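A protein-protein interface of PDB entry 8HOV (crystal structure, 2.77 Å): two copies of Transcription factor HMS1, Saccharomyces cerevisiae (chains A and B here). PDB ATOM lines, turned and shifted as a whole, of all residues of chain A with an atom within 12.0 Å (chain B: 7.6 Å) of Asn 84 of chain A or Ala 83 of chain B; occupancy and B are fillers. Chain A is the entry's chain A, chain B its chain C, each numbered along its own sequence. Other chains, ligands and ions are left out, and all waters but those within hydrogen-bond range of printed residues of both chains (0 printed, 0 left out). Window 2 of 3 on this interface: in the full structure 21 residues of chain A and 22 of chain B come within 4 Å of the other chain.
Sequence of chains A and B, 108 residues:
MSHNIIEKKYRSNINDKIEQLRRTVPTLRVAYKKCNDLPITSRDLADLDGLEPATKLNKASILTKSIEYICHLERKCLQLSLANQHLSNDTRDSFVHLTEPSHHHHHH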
ATOM      1  N   ARG A  75      14.149 -23.997 -34.739  1.00  0.00           N
ATOM      2  CA  ARG A  75      14.266 -24.371 -33.308  1.00  0.00           C
ATOM      3  C   ARG A  75      14.640 -23.144 -32.481  1.00  0.00           C
ATOM      4  O   ARG A  75      14.219 -23.065 -31.321  1.00  0.00           O
ATOM      5  CB  ARG A  75      15.350 -25.435 -33.143  1.00  0.00           C
ATOM      6  CG  ARG A  75      15.017 -26.776 -33.781  1.00  0.00           C
ATOM      7  CD  ARG A  75      14.679 -27.813 -32.730  1.00  0.00           C
ATOM      8  NE  ARG A  75      14.450 -29.136 -33.292  1.00  0.00           N
ATOM      9  CZ  ARG A  75      14.179 -30.218 -32.572  1.00  0.00           C
ATOM     10  NH1 ARG A  75      14.106 -30.136 -31.256  1.00  0.00           N
ATOM     11  NH2 ARG A  75      13.985 -31.380 -33.171  1.00  0.00           N
ATOM     12  N   LYS A  76      15.424 -22.240 -33.054  1.00  0.00           N
ATOM     13  CA  LYS A  76      15.903 -21.073 -32.283  1.00  0.00           C
ATOM     14  C   LYS A  76      14.820 -20.005 -32.276  1.00  0.00           C
ATOM     15  O   LYS A  76      14.954 -19.043 -31.511  1.00  0.00           O
ATOM     16  CB  LYS A  76      17.196 -20.514 -32.881  1.00  0.00           C
ATOM     17  CG  LYS A  76      17.845 -19.390 -32.087  1.00  0.00           C
ATOM     18  CD  LYS A  76      19.171 -18.944 -32.657  1.00  0.00           C
ATOM     19  CE  LYS A  76      19.055 -18.384 -34.057  1.00  0.00           C
ATOM     20  NZ  LYS A  76      20.359 -17.890 -34.557  1.00  0.00           N
ATOM     21  N   CYS A  77      13.790 -20.162 -33.096  1.00  0.00           N
ATOM     22  CA  CYS A  77      12.695 -19.170 -33.011  1.00  0.00           C
ATOM     23  C   CYS A  77      11.739 -19.603 -31.905  1.00  0.00           C
ATOM     24  O   CYS A  77      11.252 -18.738 -31.175  1.00  0.00           O
ATOM     25  CB  CYS A  77      11.951 -19.046 -34.333  1.00  0.00           C
ATOM     26  SG  CYS A  77      12.971 -18.385 -35.675  1.00  0.00           S
ATOM     27  N   LEU A  78      11.477 -20.901 -31.805  1.00  0.00           N
ATOM     28  CA  LEU A  78      10.578 -21.405 -30.741  1.00  0.00           C
ATOM     29  C   LEU A  78      11.176 -21.004 -29.397  1.00  0.00           C
ATOM     30  O   LEU A  78      10.568 -20.175 -28.701  1.00  0.00           O
ATOM     31  CB  LEU A  78      10.454 -22.924 -30.862  1.00  0.00           C
ATOM     32  CG  LEU A  78       9.320 -23.555 -30.062  1.00  0.00           C
ATOM     33  CD1 LEU A  78       8.020 -22.812 -30.308  1.00  0.00           C
ATOM     34  CD2 LEU A  78       9.172 -25.025 -30.415  1.00  0.00           C
ATOM     35  N   GLN A  79      12.336 -21.565 -29.063  1.00  0.00           N
ATOM     36  CA  GLN A  79      13.017 -21.219 -27.797  1.00  0.00           C
ATOM     37  C   GLN A  79      12.942 -19.711 -27.590  1.00  0.00           C
ATOM     38  O   GLN A  79      12.362 -19.283 -26.587  1.00  0.00           O
ATOM     39  CB  GLN A  79      14.467 -21.685 -27.864  1.00  0.00           C
ATOM     40  CG  GLN A  79      15.255 -21.408 -26.593  1.00  0.00           C
ATOM     41  CD  GLN A  79      16.180 -20.225 -26.741  1.00  0.00           C
ATOM     42  OE1 GLN A  79      16.876 -20.082 -27.743  1.00  0.00           O
ATOM     43  NE2 GLN A  79      16.205 -19.372 -25.730  1.00  0.00           N
ATOM     44  N   LEU A  80      13.500 -18.939 -28.511  1.00  0.00           N
ATOM     45  CA  LEU A  80      13.551 -17.474 -28.318  1.00  0.00           C
ATOM     46  C   LEU A  80      12.132 -16.969 -28.068  1.00  0.00           C
ATOM     47  O   LEU A  80      11.958 -16.124 -27.179  1.00  0.00           O
ATOM     48  CB  LEU A  80      14.143 -16.833 -29.575  1.00  0.00           C
ATOM     49  CG  LEU A  80      15.553 -16.267 -29.438  1.00  0.00           C
ATOM     50  CD1 LEU A  80      16.495 -17.301 -28.849  1.00  0.00           C
ATOM     51  CD2 LEU A  80      16.066 -15.787 -30.785  1.00  0.00           C
ATOM     52  N   SER A  81      11.159 -17.470 -28.825  1.00  0.00           N
ATOM     53  CA  SER A  81       9.773 -16.956 -28.698  1.00  0.00           C
ATOM     54  C   SER A  81       9.185 -17.402 -27.362  1.00  0.00           C
ATOM     55  O   SER A  81       8.638 -16.547 -26.645  1.00  0.00           O
ATOM     56  CB  SER A  81       8.926 -17.416 -29.839  1.00  0.00           C
ATOM     57  OG  SER A  81       8.769 -18.824 -29.805  1.00  0.00           O
ATOM     58  N   LEU A  82       9.327 -18.685 -27.031  1.00  0.00           N
ATOM     59  CA  LEU A  82       8.720 -19.202 -25.783  1.00  0.00           C
ATOM     60  C   LEU A  82       9.177 -18.317 -24.624  1.00  0.00           C
ATOM     61  O   LEU A  82       8.350 -17.999 -23.757  1.00  0.00           O
ATOM     62  CB  LEU A  82       9.159 -20.652 -25.589  1.00  0.00           C
ATOM     63  CG  LEU A  82       8.482 -21.669 -26.502  1.00  0.00           C
ATOM     64  CD1 LEU A  82       9.160 -23.025 -26.391  1.00  0.00           C
ATOM     65  CD2 LEU A  82       7.006 -21.784 -26.167  1.00  0.00           C
ATOM     66  N   ALA A  83      10.446 -17.921 -24.629  1.00  0.00           N
ATOM     67  CA  ALA A  83      10.984 -17.074 -23.546  1.00  0.00           C
ATOM     68  C   ALA A  83      10.339 -15.692 -23.609  1.00  0.00           C
ATOM     69  O   ALA A  83       9.935 -15.179 -22.558  1.00  0.00           O
ATOM     70  CB  ALA A  83      12.473 -16.977 -23.692  1.00  0.00           C
ATOM     71  N   ASN A  84      10.266 -15.115 -24.803  1.00  0.00           N
ATOM     72  CA  ASN A  84       9.670 -13.793 -24.966  1.00  0.00           C
ATOM     73  C   ASN A  84       8.261 -13.747 -24.388  1.00  0.00           C
ATOM     74  O   ASN A  84       7.872 -12.759 -23.756  1.00  0.00           O
ATOM     75  CB  ASN A  84       9.658 -13.399 -26.443  1.00  0.00           C
ATOM     76  CG  ASN A  84       9.386 -11.920 -26.649  1.00  0.00           C
ATOM     77  OD1 ASN A  84       9.795 -11.085 -25.841  1.00  0.00           O
ATOM     78  ND2 ASN A  84       8.689 -11.589 -27.729  1.00  0.00           N
ATOM     79  N   GLN A  85       7.480 -14.807 -24.594  1.00  0.00           N
ATOM     80  CA  GLN A  85       6.128 -14.896 -24.055  1.00  0.00           C
ATOM     81  C   GLN A  85       6.100 -15.379 -22.610  1.00  0.00           C
ATOM     82  O   GLN A  85       5.012 -15.617 -22.073  1.00  0.00           O
ATOM     83  CB  GLN A  85       5.270 -15.816 -24.929  1.00  0.00           C
ATOM     84  CG  GLN A  85       5.176 -15.381 -26.382  1.00  0.00           C
ATOM     85  CD  GLN A  85       4.630 -13.977 -26.533  1.00  0.00           C
ATOM     86  OE1 GLN A  85       3.515 -13.683 -26.102  1.00  0.00           O
ATOM     87  NE2 GLN A  85       5.418 -13.099 -27.141  1.00  0.00           N
ATOM     88  N   HIS A  86       7.269 -15.529 -21.982  1.00  0.00           N
ATOM     89  CA  HIS A  86       7.390 -15.958 -20.588  1.00  0.00           C
ATOM     90  C   HIS A  86       6.758 -17.328 -20.358  1.00  0.00           C
ATOM     91  O   HIS A  86       6.205 -17.600 -19.290  1.00  0.00           O
ATOM     92  CB  HIS A  86       6.789 -14.921 -19.633  1.00  0.00           C
ATOM     93  CG  HIS A  86       7.248 -13.521 -19.896  1.00  0.00           C
ATOM     94  ND1 HIS A  86       8.530 -13.094 -19.624  1.00  0.00           N
ATOM     95  CD2 HIS A  86       6.596 -12.449 -20.406  1.00  0.00           C
ATOM     96  CE1 HIS A  86       8.648 -11.821 -19.956  1.00  0.00           C
ATOM     97  NE2 HIS A  86       7.488 -11.405 -20.434  1.00  0.00           N
ATOM     98  N   LEU A  87       6.835 -18.203 -21.360  1.00  0.00           N
ATOM     99  CA  LEU A  87       6.340 -19.569 -21.220  1.00  0.00           C
ATOM    100  C   LEU A  87       7.457 -20.514 -20.787  1.00  0.00           C
ATOM    101  O   LEU A  87       7.384 -21.118 -19.711  1.00  0.00           O
ATOM    102  CB  LEU A  87       5.707 -20.032 -22.537  1.00  0.00           C
ATOM    103  CG  LEU A  87       4.413 -19.328 -22.955  1.00  0.00           C
ATOM    104  CD1 LEU A  87       4.261 -19.337 -24.462  1.00  0.00           C
ATOM    105  CD2 LEU A  87       3.214 -19.992 -22.303  1.00  0.00           C
ATOM    106  N   SER A  88       8.499 -20.630 -21.607  1.00  0.00           N
ATOM    107  CA  SER A  88       9.694 -21.413 -21.290  1.00  0.00           C
ATOM    108  C   SER A  88       9.383 -22.822 -20.787  1.00  0.00           C
ATOM    109  O   SER A  88       9.770 -23.193 -19.678  1.00  0.00           O
ATOM    110  CB  SER A  88      10.543 -20.671 -20.255  1.00  0.00           C
ATOM    111  OG  SER A  88      10.958 -19.411 -20.758  1.00  0.00           O
ATOM    112  N   CYS B  77      14.480 -14.329 -35.759  1.00  0.00           N
ATOM    113  CA  CYS B  77      15.337 -14.665 -34.600  1.00  0.00           C
ATOM    114  C   CYS B  77      15.979 -13.380 -34.098  1.00  0.00           C
ATOM    115  O   CYS B  77      15.965 -13.159 -32.896  1.00  0.00           O
ATOM    116  CB  CYS B  77      16.425 -15.647 -34.997  1.00  0.00           C
ATOM    117  SG  CYS B  77      15.791 -17.248 -35.556  1.00  0.00           S
ATOM    118  N   LEU B  78      16.492 -12.558 -35.005  1.00  0.00           N
ATOM    119  CA  LEU B  78      17.200 -11.337 -34.561  1.00  0.00           C
ATOM    120  C   LEU B  78      16.239 -10.497 -33.723  1.00  0.00           C
ATOM    121  O   LEU B  78      16.579 -10.204 -32.576  1.00  0.00           O
ATOM    122  CB  LEU B  78      17.680 -10.559 -35.787  1.00  0.00           C
ATOM    123  CG  LEU B  78      18.247  -9.171 -35.498  1.00  0.00           C
ATOM    124  CD1 LEU B  78      19.423  -9.260 -34.540  1.00  0.00           C
ATOM    125  CD2 LEU B  78      18.660  -8.478 -36.784  1.00  0.00           C
ATOM    126  N   GLN B  79      15.066 -10.170 -34.263  1.00  0.00           N
ATOM    127  CA  GLN B  79      14.143  -9.272 -33.525  1.00  0.00           C
ATOM    128  C   GLN B  79      13.751  -9.918 -32.198  1.00  0.00           C
ATOM    129  O   GLN B  79      13.665  -9.194 -31.204  1.00  0.00           O
ATOM    130  CB  GLN B  79      12.905  -8.970 -34.361  1.00  0.00           C
ATOM    131  CG  GLN B  79      11.898  -8.092 -33.637  1.00  0.00           C
ATOM    132  CD  GLN B  79      12.550  -6.855 -33.072  1.00  0.00           C
ATOM    133  OE1 GLN B  79      12.549  -6.628 -31.864  1.00  0.00           O
ATOM    134  NE2 GLN B  79      13.129  -6.049 -33.946  1.00  0.00           N
ATOM    135  N   LEU B  80      13.526 -11.229 -32.188  1.00  0.00           N
ATOM    136  CA  LEU B  80      13.079 -11.917 -30.953  1.00  0.00           C
ATOM    137  C   LEU B  80      14.169 -11.791 -29.891  1.00  0.00           C
ATOM    138  O   LEU B  80      13.848 -11.427 -28.747  1.00  0.00           O
ATOM    139  CB  LEU B  80      12.817 -13.387 -31.281  1.00  0.00           C
ATOM    140  CG  LEU B  80      11.500 -13.690 -31.990  1.00  0.00           C
ATOM    141  CD1 LEU B  80      11.394 -15.173 -32.304  1.00  0.00           C
ATOM    142  CD2 LEU B  80      10.321 -13.247 -31.139  1.00  0.00           C
ATOM    143  N   SER B  81      15.414 -12.067 -30.266  1.00  0.00           N
ATOM    144  CA  SER B  81      16.543 -12.006 -29.312  1.00  0.00           C
ATOM    145  C   SER B  81      16.720 -10.566 -28.844  1.00  0.00           C
ATOM    146  O   SER B  81      17.084 -10.356 -27.672  1.00  0.00           O
ATOM    147  CB  SER B  81      17.782 -12.528 -29.957  1.00  0.00           C
ATOM    148  OG  SER B  81      17.949 -11.954 -31.243  1.00  0.00           O
ATOM    149  N   LEU B  82      16.455  -9.613 -29.728  1.00  0.00           N
ATOM    150  CA  LEU B  82      16.552  -8.196 -29.317  1.00  0.00           C
ATOM    151  C   LEU B  82      15.502  -7.938 -28.237  1.00  0.00           C
ATOM    152  O   LEU B  82      15.783  -7.145 -27.323  1.00  0.00           O
ATOM    153  CB  LEU B  82      16.354  -7.294 -30.537  1.00  0.00           C
ATOM    154  CG  LEU B  82      17.630  -6.690 -31.113  1.00  0.00           C
ATOM    155  CD1 LEU B  82      18.615  -7.779 -31.498  1.00  0.00           C
ATOM    156  CD2 LEU B  82      17.318  -5.807 -32.309  1.00  0.00           C
ATOM    157  N   ALA B  83      14.353  -8.611 -28.318  1.00  0.00           N
ATOM    158  CA  ALA B  83      13.376  -8.430 -27.249  1.00  0.00           C
ATOM    159  C   ALA B  83      13.789  -9.176 -25.986  1.00  0.00           C
ATOM    160  O   ALA B  83      13.611  -8.667 -24.874  1.00  0.00           O
ATOM    161  CB  ALA B  83      11.995  -8.889 -27.717  1.00  0.00           C
ATOM    162  N   ASN B  84      14.333 -10.387 -26.137  1.00  0.00           N
ATOM    163  CA  ASN B  84      14.734 -11.172 -24.973  1.00  0.00           C
ATOM    164  C   ASN B  84      15.847 -10.479 -24.196  1.00  0.00           C
ATOM    165  O   ASN B  84      15.798 -10.391 -22.964  1.00  0.00           O
ATOM    166  CB  ASN B  84      15.169 -12.571 -25.408  1.00  0.00           C
ATOM    167  CG  ASN B  84      14.016 -13.401 -25.931  1.00  0.00           C
ATOM    168  OD1 ASN B  84      12.942 -12.875 -26.229  1.00  0.00           O
ATOM    169  ND2 ASN B  84      14.230 -14.706 -26.046  1.00  0.00           N
ATOM    170  N   GLN B  85      16.858  -9.975 -24.901  1.00  0.00           N
ATOM    171  CA  GLN B  85      17.940  -9.233 -24.265  1.00  0.00           C
ATOM    172  C   GLN B  85      17.569  -7.783 -23.978  1.00  0.00           C
ATOM    173  O   GLN B  85      18.443  -7.007 -23.572  1.00  0.00           O
ATOM    174  CB  GLN B  85      19.203  -9.288 -25.131  1.00  0.00           C
ATOM    175  CG  GLN B  85      20.111 -10.479 -24.847  1.00  0.00           C
ATOM    176  CD  GLN B  85      19.469 -11.808 -25.191  1.00  0.00           C
ATOM    177  OE1 GLN B  85      19.263 -12.655 -24.320  1.00  0.00           O
ATOM    178  NE2 GLN B  85      19.156 -12.003 -26.466  1.00  0.00           N
ATOM    179  N   HIS B  86      16.303  -7.409 -24.178  1.00  0.00           N
ATOM    180  CA  HIS B  86      15.806  -6.060 -23.910  1.00  0.00           C
ATOM    181  C   HIS B  86      16.605  -5.016 -24.695  1.00  0.00           C
ATOM    182  O   HIS B  86      17.216  -4.104 -24.137  1.00  0.00           O
ATOM    183  CB  HIS B  86      15.818  -5.762 -22.408  1.00  0.00           C
ATOM    184  CG  HIS B  86      15.012  -6.729 -21.598  1.00  0.00           C
ATOM    185  ND1 HIS B  86      13.688  -6.998 -21.867  1.00  0.00           N
ATOM    186  CD2 HIS B  86      15.343  -7.491 -20.529  1.00  0.00           C
ATOM    187  CE1 HIS B  86      13.237  -7.887 -20.998  1.00  0.00           C
ATOM    188  NE2 HIS B  86      14.221  -8.201 -20.175  1.00  0.00           N
ATOM    189  N   LEU B  87      16.584  -5.175 -26.018  1.00  0.00           N
ATOM    190  CA  LEU B  87      17.299  -4.287 -26.921  1.00  0.00           C
ATOM    191  C   LEU B  87      16.413  -3.657 -27.985  1.00  0.00           C
ATOM    192  O   LEU B  87      16.839  -2.683 -28.618  1.00  0.00           O
ATOM    193  CB  LEU B  87      18.447  -5.040 -27.612  1.00  0.00           C
ATOM    194  CG  LEU B  87      19.398  -5.833 -26.710  1.00  0.00           C
ATOM    195  CD1 LEU B  87      20.273  -6.747 -27.544  1.00  0.00           C
ATOM    196  CD2 LEU B  87      20.255  -4.906 -25.864  1.00  0.00           C
ATOM    197  N   SER B  88      15.206  -4.174 -28.197  1.00  0.00           N
ATOM    198  CA  SER B  88      14.302  -3.643 -29.212  1.00  0.00           C
ATOM    199  C   SER B  88      13.783  -2.260 -28.834  1.00  0.00           C
ATOM    200  O   SER B  88      13.234  -2.065 -27.750  1.00  0.00           O
ATOM    201  CB  SER B  88      13.129  -4.602 -29.430  1.00  0.00           C
ATOM    202  OG  SER B  88      12.461  -4.873 -28.209  1.00  0.00           O
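The backbone carbonyl oxygen (O) of Leu 80 of chain A lies within hydrogen-bond range of the side-chain amide nitrogen (ND2) of Asn 84 of chain B (2.9 Å).
The side-chain sulfur of Cys 77 of chain A lies close to the side-chain sulfur of Cys 77 of chain B (3.0 Å).
O of Cys 77 of chain A sits at hydrogen-bond distance from OG of Ser 81 of chain A.
The backbone carbonyl oxygen of Cys 77 of chain B lies within hydrogen-bond range of the side-chain hydroxyl of Ser 81 of chain B, 2.8 Å away.
O of Leu 78 of chain B sits at hydrogen-bond distance from OG of Ser 81 of chain B, at 2.6 Å.
OD1 of Asn 84 of chain B sits close to O of Leu 80 of chain B (3.0 Å).
NE2 of Gln 85 of chain B lies within hydrogen-bond range of O of Ser 81 of chain B (2.9 Å).
The backbone carbonyl oxygen (O) of Ala 83 of chain B is in hydrogen-bond range of a ring nitrogen (ND1) of His 86 of chain B (3.4 Å).
Lys 76 of chain A touches Cys 77 of chain B (CE to SG, 3.8 Å).
Cys 77 of chain A touches Leu 80 of chain B (O to CD1, 3.7 Å).
Leu 80 of chain A touches Cys 77 of chain B (CD2 to O, 3.4 Å).
Leu 80 of chain A touches Ser 81 of chain B (CD2 to CB, 3.8 Å).
Asn 84 of chain B touches Ala 83 of chain A.
Ala 83 of chain B touches Asn 84 of chain A.
CB of Asn 84 of chain A touches OD1 of Asn 84 of chain B, 3.3 Å away.
Of the printed residues of chain B, Lys 76 of chain A touches Cys 77.
Printed residues of chain B within 4 Å of Cys 77 of chain A: Cys 77 and Leu 80.
Gln 79 of chain A touches none of the printed residues of chain B.
Of the printed residues of chain B, Leu 80 of chain A touches Cys 77 (3.4 Å), Ser 81 (3.8 Å) and Asn 84 (2.9 Å).
Of chain B, only Ala 83 (3.6 Å) and Asn 84 (3.3 Å) come within 4 Å of Asn 84 of chain A.
Printed residues of chain A within 4 Å of Cys 77 of chain B: Lys 76, Cys 77 and Leu 80.
No residue of chain A comes within 4 Å of Gln 79 of chain B.
Ser 81 of chain B touches one residue of chain A.
No residue of chain A comes within 4 Å of Leu 82 of chain B.
Ala 83 of chain B touches just one residue of chain A: Asn 84.
Of chain A, only Leu 80, Ala 83 and Asn 84 come within 4 Å of Asn 84 of chain B.
No residue of chain A comes within 4 Å of Leu 87 of chain B.
No residue of chain A comes within 4 Å of Ser 88 of chain B.
Hydrophobic or aromatic side chains of chain B within 4 Å of the printed part of chain A: Leu 80 and Ala 83.
Of the 14 printed residues of chain A, 5 touch a printed residue of chain B.
Hydrophobic or aromatic side chains of chain A that line the printed part of chain B: Leu 80 and Ala 83.
Cys 77 of chain B touches its own counterpart, Cys 77 of chain A.
Cys 77 of chain A touches Leu 80 of chain B, and with the chains exchanged Leu 80 of chain A touches Cys 77 of chain B.
Leu 80 of chain A touches Asn 84 of chain B, but with the chains exchanged Asn 84 of chain A does not touch Leu 80 of chain B (4.1 Å).
Ala 83 of chain A touches Asn 84 of chain B, and with the chains exchanged Asn 84 of chain A touches Ala 83 of chain B.
12 positions are printed for both chains.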
